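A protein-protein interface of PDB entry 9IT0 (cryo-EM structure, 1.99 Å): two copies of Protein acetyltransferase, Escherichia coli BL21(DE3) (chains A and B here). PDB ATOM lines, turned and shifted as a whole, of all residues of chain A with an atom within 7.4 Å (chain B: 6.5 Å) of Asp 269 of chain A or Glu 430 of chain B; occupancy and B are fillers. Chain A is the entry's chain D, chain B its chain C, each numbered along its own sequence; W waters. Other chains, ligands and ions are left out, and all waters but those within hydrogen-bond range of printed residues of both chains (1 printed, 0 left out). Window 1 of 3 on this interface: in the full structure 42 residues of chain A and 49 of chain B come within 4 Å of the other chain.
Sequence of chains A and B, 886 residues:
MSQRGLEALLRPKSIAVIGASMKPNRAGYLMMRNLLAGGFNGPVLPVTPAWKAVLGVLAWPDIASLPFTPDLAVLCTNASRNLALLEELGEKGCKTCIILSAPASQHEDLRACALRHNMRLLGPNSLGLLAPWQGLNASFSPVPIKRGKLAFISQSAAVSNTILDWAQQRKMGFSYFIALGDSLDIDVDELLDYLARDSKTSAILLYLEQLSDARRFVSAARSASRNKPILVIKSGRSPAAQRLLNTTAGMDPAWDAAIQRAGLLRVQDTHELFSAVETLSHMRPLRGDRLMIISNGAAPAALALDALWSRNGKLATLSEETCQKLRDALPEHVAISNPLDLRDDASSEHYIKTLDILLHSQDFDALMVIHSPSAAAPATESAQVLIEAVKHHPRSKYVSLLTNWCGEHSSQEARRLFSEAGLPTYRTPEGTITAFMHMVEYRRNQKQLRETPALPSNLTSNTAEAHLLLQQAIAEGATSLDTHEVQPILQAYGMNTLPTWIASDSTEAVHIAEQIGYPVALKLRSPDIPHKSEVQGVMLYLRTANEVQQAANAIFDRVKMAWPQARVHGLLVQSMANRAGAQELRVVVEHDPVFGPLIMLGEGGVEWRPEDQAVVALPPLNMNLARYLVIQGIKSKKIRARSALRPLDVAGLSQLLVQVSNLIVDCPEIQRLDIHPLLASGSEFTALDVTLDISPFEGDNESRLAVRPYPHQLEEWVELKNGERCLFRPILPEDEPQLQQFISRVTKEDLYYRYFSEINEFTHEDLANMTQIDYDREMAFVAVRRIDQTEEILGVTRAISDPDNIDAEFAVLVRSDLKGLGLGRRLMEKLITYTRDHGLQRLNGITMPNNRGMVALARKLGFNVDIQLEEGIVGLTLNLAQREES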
ATOM      1  N   ILE A 233     -17.600   7.089   6.533  1.00  0.00           N
ATOM      2  CA  ILE A 233     -18.949   6.990   7.084  1.00  0.00           C
ATOM      3  C   ILE A 233     -19.134   8.097   8.116  1.00  0.00           C
ATOM      4  O   ILE A 233     -18.250   8.337   8.947  1.00  0.00           O
ATOM      5  CB  ILE A 233     -19.228   5.609   7.717  1.00  0.00           C
ATOM      6  CG1 ILE A 233     -20.637   5.585   8.321  1.00  0.00           C
ATOM      7  CG2 ILE A 233     -18.195   5.274   8.786  1.00  0.00           C
ATOM      8  CD1 ILE A 233     -21.251   4.204   8.411  1.00  0.00           C
ATOM      9  N   ARG A 237     -27.584  12.109  11.135  1.00  0.00           N
ATOM     10  CA  ARG A 237     -28.376  12.709  10.070  1.00  0.00           C
ATOM     11  C   ARG A 237     -29.761  13.163  10.516  1.00  0.00           C
ATOM     12  O   ARG A 237     -30.470  13.790   9.722  1.00  0.00           O
ATOM     13  CB  ARG A 237     -28.533  11.722   8.907  1.00  0.00           C
ATOM     14  CG  ARG A 237     -27.232  11.087   8.434  1.00  0.00           C
ATOM     15  CD  ARG A 237     -27.494   9.914   7.504  1.00  0.00           C
ATOM     16  NE  ARG A 237     -27.538  10.341   6.108  1.00  0.00           N
ATOM     17  CZ  ARG A 237     -26.793   9.843   5.129  1.00  0.00           C
ATOM     18  NH1 ARG A 237     -25.945   8.848   5.335  1.00  0.00           N
ATOM     19  NH2 ARG A 237     -26.905  10.354   3.907  1.00  0.00           N
ATOM     20  N   ARG A 266     -18.910   8.218   0.139  1.00  0.00           N
ATOM     21  CA  ARG A 266     -19.605   8.045   1.410  1.00  0.00           C
ATOM     22  C   ARG A 266     -20.321   6.698   1.467  1.00  0.00           C
ATOM     23  O   ARG A 266     -21.003   6.300   0.517  1.00  0.00           O
ATOM     24  CB  ARG A 266     -20.615   9.176   1.623  1.00  0.00           C
ATOM     25  CG  ARG A 266     -21.246   9.203   3.010  1.00  0.00           C
ATOM     26  CD  ARG A 266     -22.235  10.359   3.163  1.00  0.00           C
ATOM     27  NE  ARG A 266     -22.750  10.464   4.525  1.00  0.00           N
ATOM     28  CZ  ARG A 266     -23.574  11.414   4.951  1.00  0.00           C
ATOM     29  NH1 ARG A 266     -24.005  12.371   4.147  1.00  0.00           N
ATOM     30  NH2 ARG A 266     -23.976  11.402   6.218  1.00  0.00           N
ATOM     31  N   VAL A 267     -20.171   6.007   2.597  1.00  0.00           N
ATOM     32  CA  VAL A 267     -20.829   4.728   2.855  1.00  0.00           C
ATOM     33  C   VAL A 267     -21.971   4.961   3.840  1.00  0.00           C
ATOM     34  O   VAL A 267     -21.920   5.873   4.673  1.00  0.00           O
ATOM     35  CB  VAL A 267     -19.806   3.691   3.378  1.00  0.00           C
ATOM     36  CG1 VAL A 267     -20.395   2.810   4.480  1.00  0.00           C
ATOM     37  CG2 VAL A 267     -19.271   2.840   2.222  1.00  0.00           C
ATOM     38  N   GLN A 268     -23.009   4.125   3.746  1.00  0.00           N
ATOM     39  CA  GLN A 268     -24.306   4.455   4.333  1.00  0.00           C
ATOM     40  C   GLN A 268     -24.523   3.896   5.742  1.00  0.00           C
ATOM     41  O   GLN A 268     -25.008   4.620   6.616  1.00  0.00           O
ATOM     42  CB  GLN A 268     -25.427   3.966   3.411  1.00  0.00           C
ATOM     43  CG  GLN A 268     -25.415   4.595   2.021  1.00  0.00           C
ATOM     44  CD  GLN A 268     -25.337   6.112   2.057  1.00  0.00           C
ATOM     45  OE1 GLN A 268     -26.169   6.773   2.676  1.00  0.00           O
ATOM     46  NE2 GLN A 268     -24.324   6.667   1.403  1.00  0.00           N
ATOM     47  N   ASP A 269     -24.197   2.626   5.991  1.00  0.00           N
ATOM     48  CA  ASP A 269     -24.570   1.999   7.256  1.00  0.00           C
ATOM     49  C   ASP A 269     -23.536   0.951   7.659  1.00  0.00           C
ATOM     50  O   ASP A 269     -22.519   0.758   6.989  1.00  0.00           O
ATOM     51  CB  ASP A 269     -25.979   1.393   7.166  1.00  0.00           C
ATOM     52  CG  ASP A 269     -26.093   0.313   6.102  1.00  0.00           C
ATOM     53  OD1 ASP A 269     -25.079  -0.343   5.787  1.00  0.00           O
ATOM     54  OD2 ASP A 269     -27.210   0.119   5.581  1.00  0.00           O
ATOM     55  N   THR A 270     -23.820   0.267   8.774  1.00  0.00           N
ATOM     56  CA  THR A 270     -22.841  -0.625   9.395  1.00  0.00           C
ATOM     57  C   THR A 270     -22.459  -1.783   8.479  1.00  0.00           C
ATOM     58  O   THR A 270     -21.279  -2.142   8.387  1.00  0.00           O
ATOM     59  CB  THR A 270     -23.390  -1.156  10.725  1.00  0.00           C
ATOM     60  OG1 THR A 270     -23.734  -0.058  11.581  1.00  0.00           O
ATOM     61  CG2 THR A 270     -22.362  -2.035  11.434  1.00  0.00           C
ATOM     62  N   HIS A 271     -23.437  -2.393   7.804  1.00  0.00           N
ATOM     63  CA  HIS A 271     -23.130  -3.523   6.928  1.00  0.00           C
ATOM     64  C   HIS A 271     -22.152  -3.106   5.835  1.00  0.00           C
ATOM     65  O   HIS A 271     -21.154  -3.794   5.566  1.00  0.00           O
ATOM     66  CB  HIS A 271     -24.419  -4.061   6.304  1.00  0.00           C
ATOM     67  CG  HIS A 271     -25.083  -5.140   7.103  1.00  0.00           C
ATOM     68  ND1 HIS A 271     -26.451  -5.204   7.263  1.00  0.00           N
ATOM     69  CD2 HIS A 271     -24.574  -6.190   7.787  1.00  0.00           C
ATOM     70  CE1 HIS A 271     -26.756  -6.250   8.010  1.00  0.00           C
ATOM     71  NE2 HIS A 271     -25.635  -6.865   8.342  1.00  0.00           N
ATOM     72  N   GLU A 272     -22.426  -1.964   5.202  1.00  0.00           N
ATOM     73  CA  GLU A 272     -21.551  -1.462   4.151  1.00  0.00           C
ATOM     74  C   GLU A 272     -20.150  -1.178   4.676  1.00  0.00           C
ATOM     75  O   GLU A 272     -19.181  -1.301   3.927  1.00  0.00           O
ATOM     76  CB  GLU A 272     -22.168  -0.212   3.522  1.00  0.00           C
ATOM     77  CG  GLU A 272     -23.511  -0.464   2.836  1.00  0.00           C
ATOM     78  CD  GLU A 272     -23.969   0.703   1.978  1.00  0.00           C
ATOM     79  OE1 GLU A 272     -23.226   1.701   1.872  1.00  0.00           O
ATOM     80  OE2 GLU A 272     -25.074   0.620   1.402  1.00  0.00           O
ATOM     81  N   LEU A 273     -20.014  -0.833   5.960  1.00  0.00           N
ATOM     82  CA  LEU A 273     -18.686  -0.614   6.533  1.00  0.00           C
ATOM     83  C   LEU A 273     -17.880  -1.914   6.575  1.00  0.00           C
ATOM     84  O   LEU A 273     -16.699  -1.941   6.202  1.00  0.00           O
ATOM     85  CB  LEU A 273     -18.826  -0.010   7.933  1.00  0.00           C
ATOM     86  CG  LEU A 273     -17.553   0.295   8.725  1.00  0.00           C
ATOM     87  CD1 LEU A 273     -16.700   1.330   8.007  1.00  0.00           C
ATOM     88  CD2 LEU A 273     -17.900   0.774  10.128  1.00  0.00           C
ATOM     89  N   PHE A 274     -18.504  -3.004   7.032  1.00  0.00           N
ATOM     90  CA  PHE A 274     -17.831  -4.303   7.049  1.00  0.00           C
ATOM     91  C   PHE A 274     -17.441  -4.723   5.634  1.00  0.00           C
ATOM     92  O   PHE A 274     -16.311  -5.180   5.383  1.00  0.00           O
ATOM     93  CB  PHE A 274     -18.752  -5.358   7.676  1.00  0.00           C
ATOM     94  CG  PHE A 274     -19.011  -5.171   9.159  1.00  0.00           C
ATOM     95  CD1 PHE A 274     -18.175  -4.398   9.953  1.00  0.00           C
ATOM     96  CD2 PHE A 274     -20.107  -5.779   9.753  1.00  0.00           C
ATOM     97  CE1 PHE A 274     -18.431  -4.238  11.307  1.00  0.00           C
ATOM     98  CE2 PHE A 274     -20.367  -5.624  11.103  1.00  0.00           C
ATOM     99  CZ  PHE A 274     -19.527  -4.852  11.882  1.00  0.00           C
ATOM    100  N   SER A 275     -18.375  -4.572   4.691  1.00  0.00           N
ATOM    101  CA  SER A 275     -18.068  -4.913   3.307  1.00  0.00           C
ATOM    102  C   SER A 275     -16.933  -4.048   2.768  1.00  0.00           C
ATOM    103  O   SER A 275     -16.105  -4.520   1.983  1.00  0.00           O
ATOM    104  CB  SER A 275     -19.322  -4.775   2.441  1.00  0.00           C
ATOM    105  OG  SER A 275     -19.575  -3.422   2.104  1.00  0.00           O
ATOM    106  N   LEU B 303     -26.616   5.638  15.396  1.00  0.00           N
ATOM    107  CA  LEU B 303     -26.922   4.920  14.160  1.00  0.00           C
ATOM    108  C   LEU B 303     -28.338   4.350  14.198  1.00  0.00           C
ATOM    109  O   LEU B 303     -29.078   4.420  13.206  1.00  0.00           O
ATOM    110  CB  LEU B 303     -25.896   3.809  13.930  1.00  0.00           C
ATOM    111  CG  LEU B 303     -24.456   4.257  13.657  1.00  0.00           C
ATOM    112  CD1 LEU B 303     -23.485   3.115  13.905  1.00  0.00           C
ATOM    113  CD2 LEU B 303     -24.296   4.786  12.241  1.00  0.00           C
ATOM    114  N   ALA B 304     -28.738   3.795  15.346  1.00  0.00           N
ATOM    115  CA  ALA B 304     -30.103   3.295  15.480  1.00  0.00           C
ATOM    116  C   ALA B 304     -31.123   4.415  15.308  1.00  0.00           C
ATOM    117  O   ALA B 304     -32.166   4.219  14.677  1.00  0.00           O
ATOM    118  CB  ALA B 304     -30.287   2.609  16.834  1.00  0.00           C
ATOM    119  N   ALA B 307     -31.491   5.232  11.652  1.00  0.00           N
ATOM    120  CA  ALA B 307     -32.305   4.208  11.002  1.00  0.00           C
ATOM    121  C   ALA B 307     -33.784   4.389  11.332  1.00  0.00           C
ATOM    122  O   ALA B 307     -34.643   4.275  10.450  1.00  0.00           O
ATOM    123  CB  ALA B 307     -31.831   2.814  11.414  1.00  0.00           C
ATOM    124  N   ARG B 311     -37.425   5.621   8.797  1.00  0.00           N
ATOM    125  CA  ARG B 311     -38.637   4.826   8.624  1.00  0.00           C
ATOM    126  C   ARG B 311     -39.838   5.372   9.393  1.00  0.00           C
ATOM    127  O   ARG B 311     -40.846   4.670   9.515  1.00  0.00           O
ATOM    128  CB  ARG B 311     -38.377   3.376   9.036  1.00  0.00           C
ATOM    129  CG  ARG B 311     -37.368   2.659   8.161  1.00  0.00           C
ATOM    130  CD  ARG B 311     -37.026   1.286   8.710  1.00  0.00           C
ATOM    131  NE  ARG B 311     -36.154   0.539   7.811  1.00  0.00           N
ATOM    132  CZ  ARG B 311     -34.896   0.860   7.542  1.00  0.00           C
ATOM    133  NH1 ARG B 311     -34.315   1.913   8.097  1.00  0.00           N
ATOM    134  NH2 ARG B 311     -34.201   0.107   6.694  1.00  0.00           N
ATOM    135  N   MET B 368     -34.944  -2.067  23.512  1.00  0.00           N
ATOM    136  CA  MET B 368     -33.758  -2.439  22.747  1.00  0.00           C
ATOM    137  C   MET B 368     -32.520  -2.279  23.626  1.00  0.00           C
ATOM    138  O   MET B 368     -32.276  -1.191  24.159  1.00  0.00           O
ATOM    139  CB  MET B 368     -33.634  -1.574  21.492  1.00  0.00           C
ATOM    140  CG  MET B 368     -32.498  -1.966  20.561  1.00  0.00           C
ATOM    141  SD  MET B 368     -32.555  -1.078  18.988  1.00  0.00           S
ATOM    142  CE  MET B 368     -30.872  -1.287  18.408  1.00  0.00           C
ATOM    143  N   ASN B 404     -29.028  -6.707  20.820  1.00  0.00           N
ATOM    144  CA  ASN B 404     -28.078  -6.424  19.737  1.00  0.00           C
ATOM    145  C   ASN B 404     -26.682  -6.384  20.357  1.00  0.00           C
ATOM    146  O   ASN B 404     -26.267  -5.363  20.911  1.00  0.00           O
ATOM    147  CB  ASN B 404     -28.415  -5.120  19.027  1.00  0.00           C
ATOM    148  CG  ASN B 404     -27.303  -4.658  18.098  1.00  0.00           C
ATOM    149  OD1 ASN B 404     -26.629  -5.471  17.471  1.00  0.00           O
ATOM    150  ND2 ASN B 404     -27.102  -3.350  18.018  1.00  0.00           N
ATOM    151  N   THR B 428     -26.579  -6.177  13.869  1.00  0.00           N
ATOM    152  CA  THR B 428     -26.310  -4.746  13.817  1.00  0.00           C
ATOM    153  C   THR B 428     -27.541  -3.950  14.227  1.00  0.00           C
ATOM    154  O   THR B 428     -28.673  -4.407  14.041  1.00  0.00           O
ATOM    155  CB  THR B 428     -25.873  -4.308  12.406  1.00  0.00           C
ATOM    156  OG1 THR B 428     -27.017  -4.208  11.550  1.00  0.00           O
ATOM    157  CG2 THR B 428     -24.876  -5.302  11.812  1.00  0.00           C
ATOM    158  N   PRO B 429     -27.350  -2.747  14.785  1.00  0.00           N
ATOM    159  CA  PRO B 429     -28.514  -1.976  15.265  1.00  0.00           C
ATOM    160  C   PRO B 429     -29.503  -1.600  14.168  1.00  0.00           C
ATOM    161  O   PRO B 429     -30.721  -1.605  14.407  1.00  0.00           O
ATOM    162  CB  PRO B 429     -27.877  -0.737  15.913  1.00  0.00           C
ATOM    163  CG  PRO B 429     -26.487  -0.668  15.407  1.00  0.00           C
ATOM    164  CD  PRO B 429     -26.074  -2.031  14.967  1.00  0.00           C
ATOM    165  N   GLU B 430     -29.014  -1.281  12.966  1.00  0.00           N
ATOM    166  CA  GLU B 430     -29.922  -0.952  11.871  1.00  0.00           C
ATOM    167  C   GLU B 430     -30.831  -2.132  11.544  1.00  0.00           C
ATOM    168  O   GLU B 430     -32.029  -1.955  11.287  1.00  0.00           O
ATOM    169  CB  GLU B 430     -29.126  -0.524  10.635  1.00  0.00           C
ATOM    170  CG  GLU B 430     -28.426   0.828  10.774  1.00  0.00           C
ATOM    171  CD  GLU B 430     -26.927   0.707  11.008  1.00  0.00           C
ATOM    172  OE1 GLU B 430     -26.477  -0.354  11.490  1.00  0.00           O
ATOM    173  OE2 GLU B 430     -26.198   1.677  10.712  1.00  0.00           O
ATOM    174  N   GLY B 431     -30.279  -3.348  11.554  1.00  0.00           N
ATOM    175  CA  GLY B 431     -31.103  -4.525  11.334  1.00  0.00           C
ATOM    176  C   GLY B 431     -32.159  -4.706  12.408  1.00  0.00           C
ATOM    177  O   GLY B 431     -33.286  -5.112  12.120  1.00  0.00           O
ATOM    178  N   THR B 432     -31.804  -4.416  13.662  1.00  0.00           N
ATOM    179  CA  THR B 432     -32.776  -4.484  14.750  1.00  0.00           C
ATOM    180  C   THR B 432     -33.933  -3.522  14.504  1.00  0.00           C
ATOM    181  O   THR B 432     -35.112  -3.892  14.630  1.00  0.00           O
ATOM    182  CB  THR B 432     -32.085  -4.164  16.079  1.00  0.00           C
ATOM    183  OG1 THR B 432     -30.843  -4.874  16.164  1.00  0.00           O
ATOM    184  CG2 THR B 432     -32.960  -4.546  17.258  1.00  0.00           C
ATOM    185  N   ILE B 433     -33.610  -2.277  14.142  1.00  0.00           N
ATOM    186  CA  ILE B 433     -34.656  -1.296  13.863  1.00  0.00           C
ATOM    187  C   ILE B 433     -35.535  -1.771  12.707  1.00  0.00           C
ATOM    188  O   ILE B 433     -36.767  -1.652  12.755  1.00  0.00           O
ATOM    189  CB  ILE B 433     -34.032   0.086  13.577  1.00  0.00           C
ATOM    190  CG1 ILE B 433     -33.271   0.610  14.805  1.00  0.00           C
ATOM    191  CG2 ILE B 433     -35.105   1.084  13.159  1.00  0.00           C
ATOM    192  CD1 ILE B 433     -34.142   0.885  16.022  1.00  0.00           C
ATOM    193  N   THR B 434     -34.917  -2.312  11.651  1.00  0.00           N
ATOM    194  CA  THR B 434     -35.685  -2.786  10.499  1.00  0.00           C
ATOM    195  C   THR B 434     -36.630  -3.921  10.885  1.00  0.00           C
ATOM    196  O   THR B 434     -37.798  -3.944  10.468  1.00  0.00           O
ATOM    197  CB  THR B 434     -34.728  -3.240   9.391  1.00  0.00           C
ATOM    198  OG1 THR B 434     -33.963  -2.121   8.922  1.00  0.00           O
ATOM    199  CG2 THR B 434     -35.490  -3.858   8.224  1.00  0.00           C
ATOM    200  N   ALA B 435     -36.141  -4.871  11.684  1.00  0.00           N
ATOM    201  CA  ALA B 435     -36.984  -5.976  12.130  1.00  0.00           C
ATOM    202  C   ALA B 435     -38.184  -5.463  12.915  1.00  0.00           C
ATOM    203  O   ALA B 435     -39.318  -5.907  12.699  1.00  0.00           O
ATOM    204  CB  ALA B 435     -36.162  -6.950  12.972  1.00  0.00           C
HETATM  205  O   HOH W   1     -26.237  -2.283   8.972  1.00  0.00           O
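The side-chain carboxylate (OE1) of Glu 430 of chain B is in hydrogen-bond range of the side-chain hydroxyl (OG1) of Thr 270 of chain A, at 2.8 Å.
Among the printed residues, pairs that only touch across the chains: Asp 269 of chain A with Glu 430 of chain B (3.6 Å), His 271 of chain A with Thr 428 of chain B (3.9 Å) and Thr 270 of chain A with Leu 303 of chain B (3.9 Å).
Water W1 lies within hydrogen-bond range of the backbone NH of His 271 of chain A, the side-chain carboxylate of Glu 430 of chain B and the side-chain hydroxyl of Thr 428 of chain B.
No position is printed for both chains.
Of chain B, only Glu 430 comes within 4 Å of Asp 269 of chain A.
Glu 430 of chain B touches two residues of chain A.
Of the printed residues of chain A, Leu 303 of chain B touches Thr 270.
Of the printed residues of chain B, His 271 of chain A touches Thr 428.
Of the printed residues of chain A, Thr 428 of chain B touches His 271 (3.9 Å).
The nearest residue of chain B that does not touch Asp 269 of chain A is Leu 303 of chain B (5.7 Å).
The nearest printed residue of chain A that does not touch Glu 430 of chain B is Gln 268 of chain A (5.2 Å).
The nearest printed residue of chain B that does not touch Thr 270 of chain A is Thr 428 of chain B (4.1 Å).
Hydrophobic or aromatic side chains of chain A within 4 Å of the printed part of chain B: His 271.
Along chain B the printed residues that touch a printed residue of chain A span positions 303 to 430.
Among the printed residues, 4 pairs touch across the chains.
Among the printed residues, no Asp or Glu carboxylate lies within 4 Å of a Lys or Arg side-chain nitrogen of the other chain.
O of Glu 430 of chain B is in hydrogen-bond range of OG1 of Thr 434 of chain B, at 3.1 Å.
The side-chain hydroxyl (OG1) of Thr 428 of chain B is in hydrogen-bond range of the backbone NH (N) of Gly 431 of chain B (3.4 Å).
OD1 of Asp 269 of chain A lies within hydrogen-bond range of N of His 271 of chain A (3.3 Å).
N of Glu 272 of chain A is in hydrogen-bond range of OD1 of Asp 269 of chain A (3.2 Å).
O of Thr 428 of chain B lies within hydrogen-bond range of OG1 of Thr 432 of chain B, at 3.1 Å.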
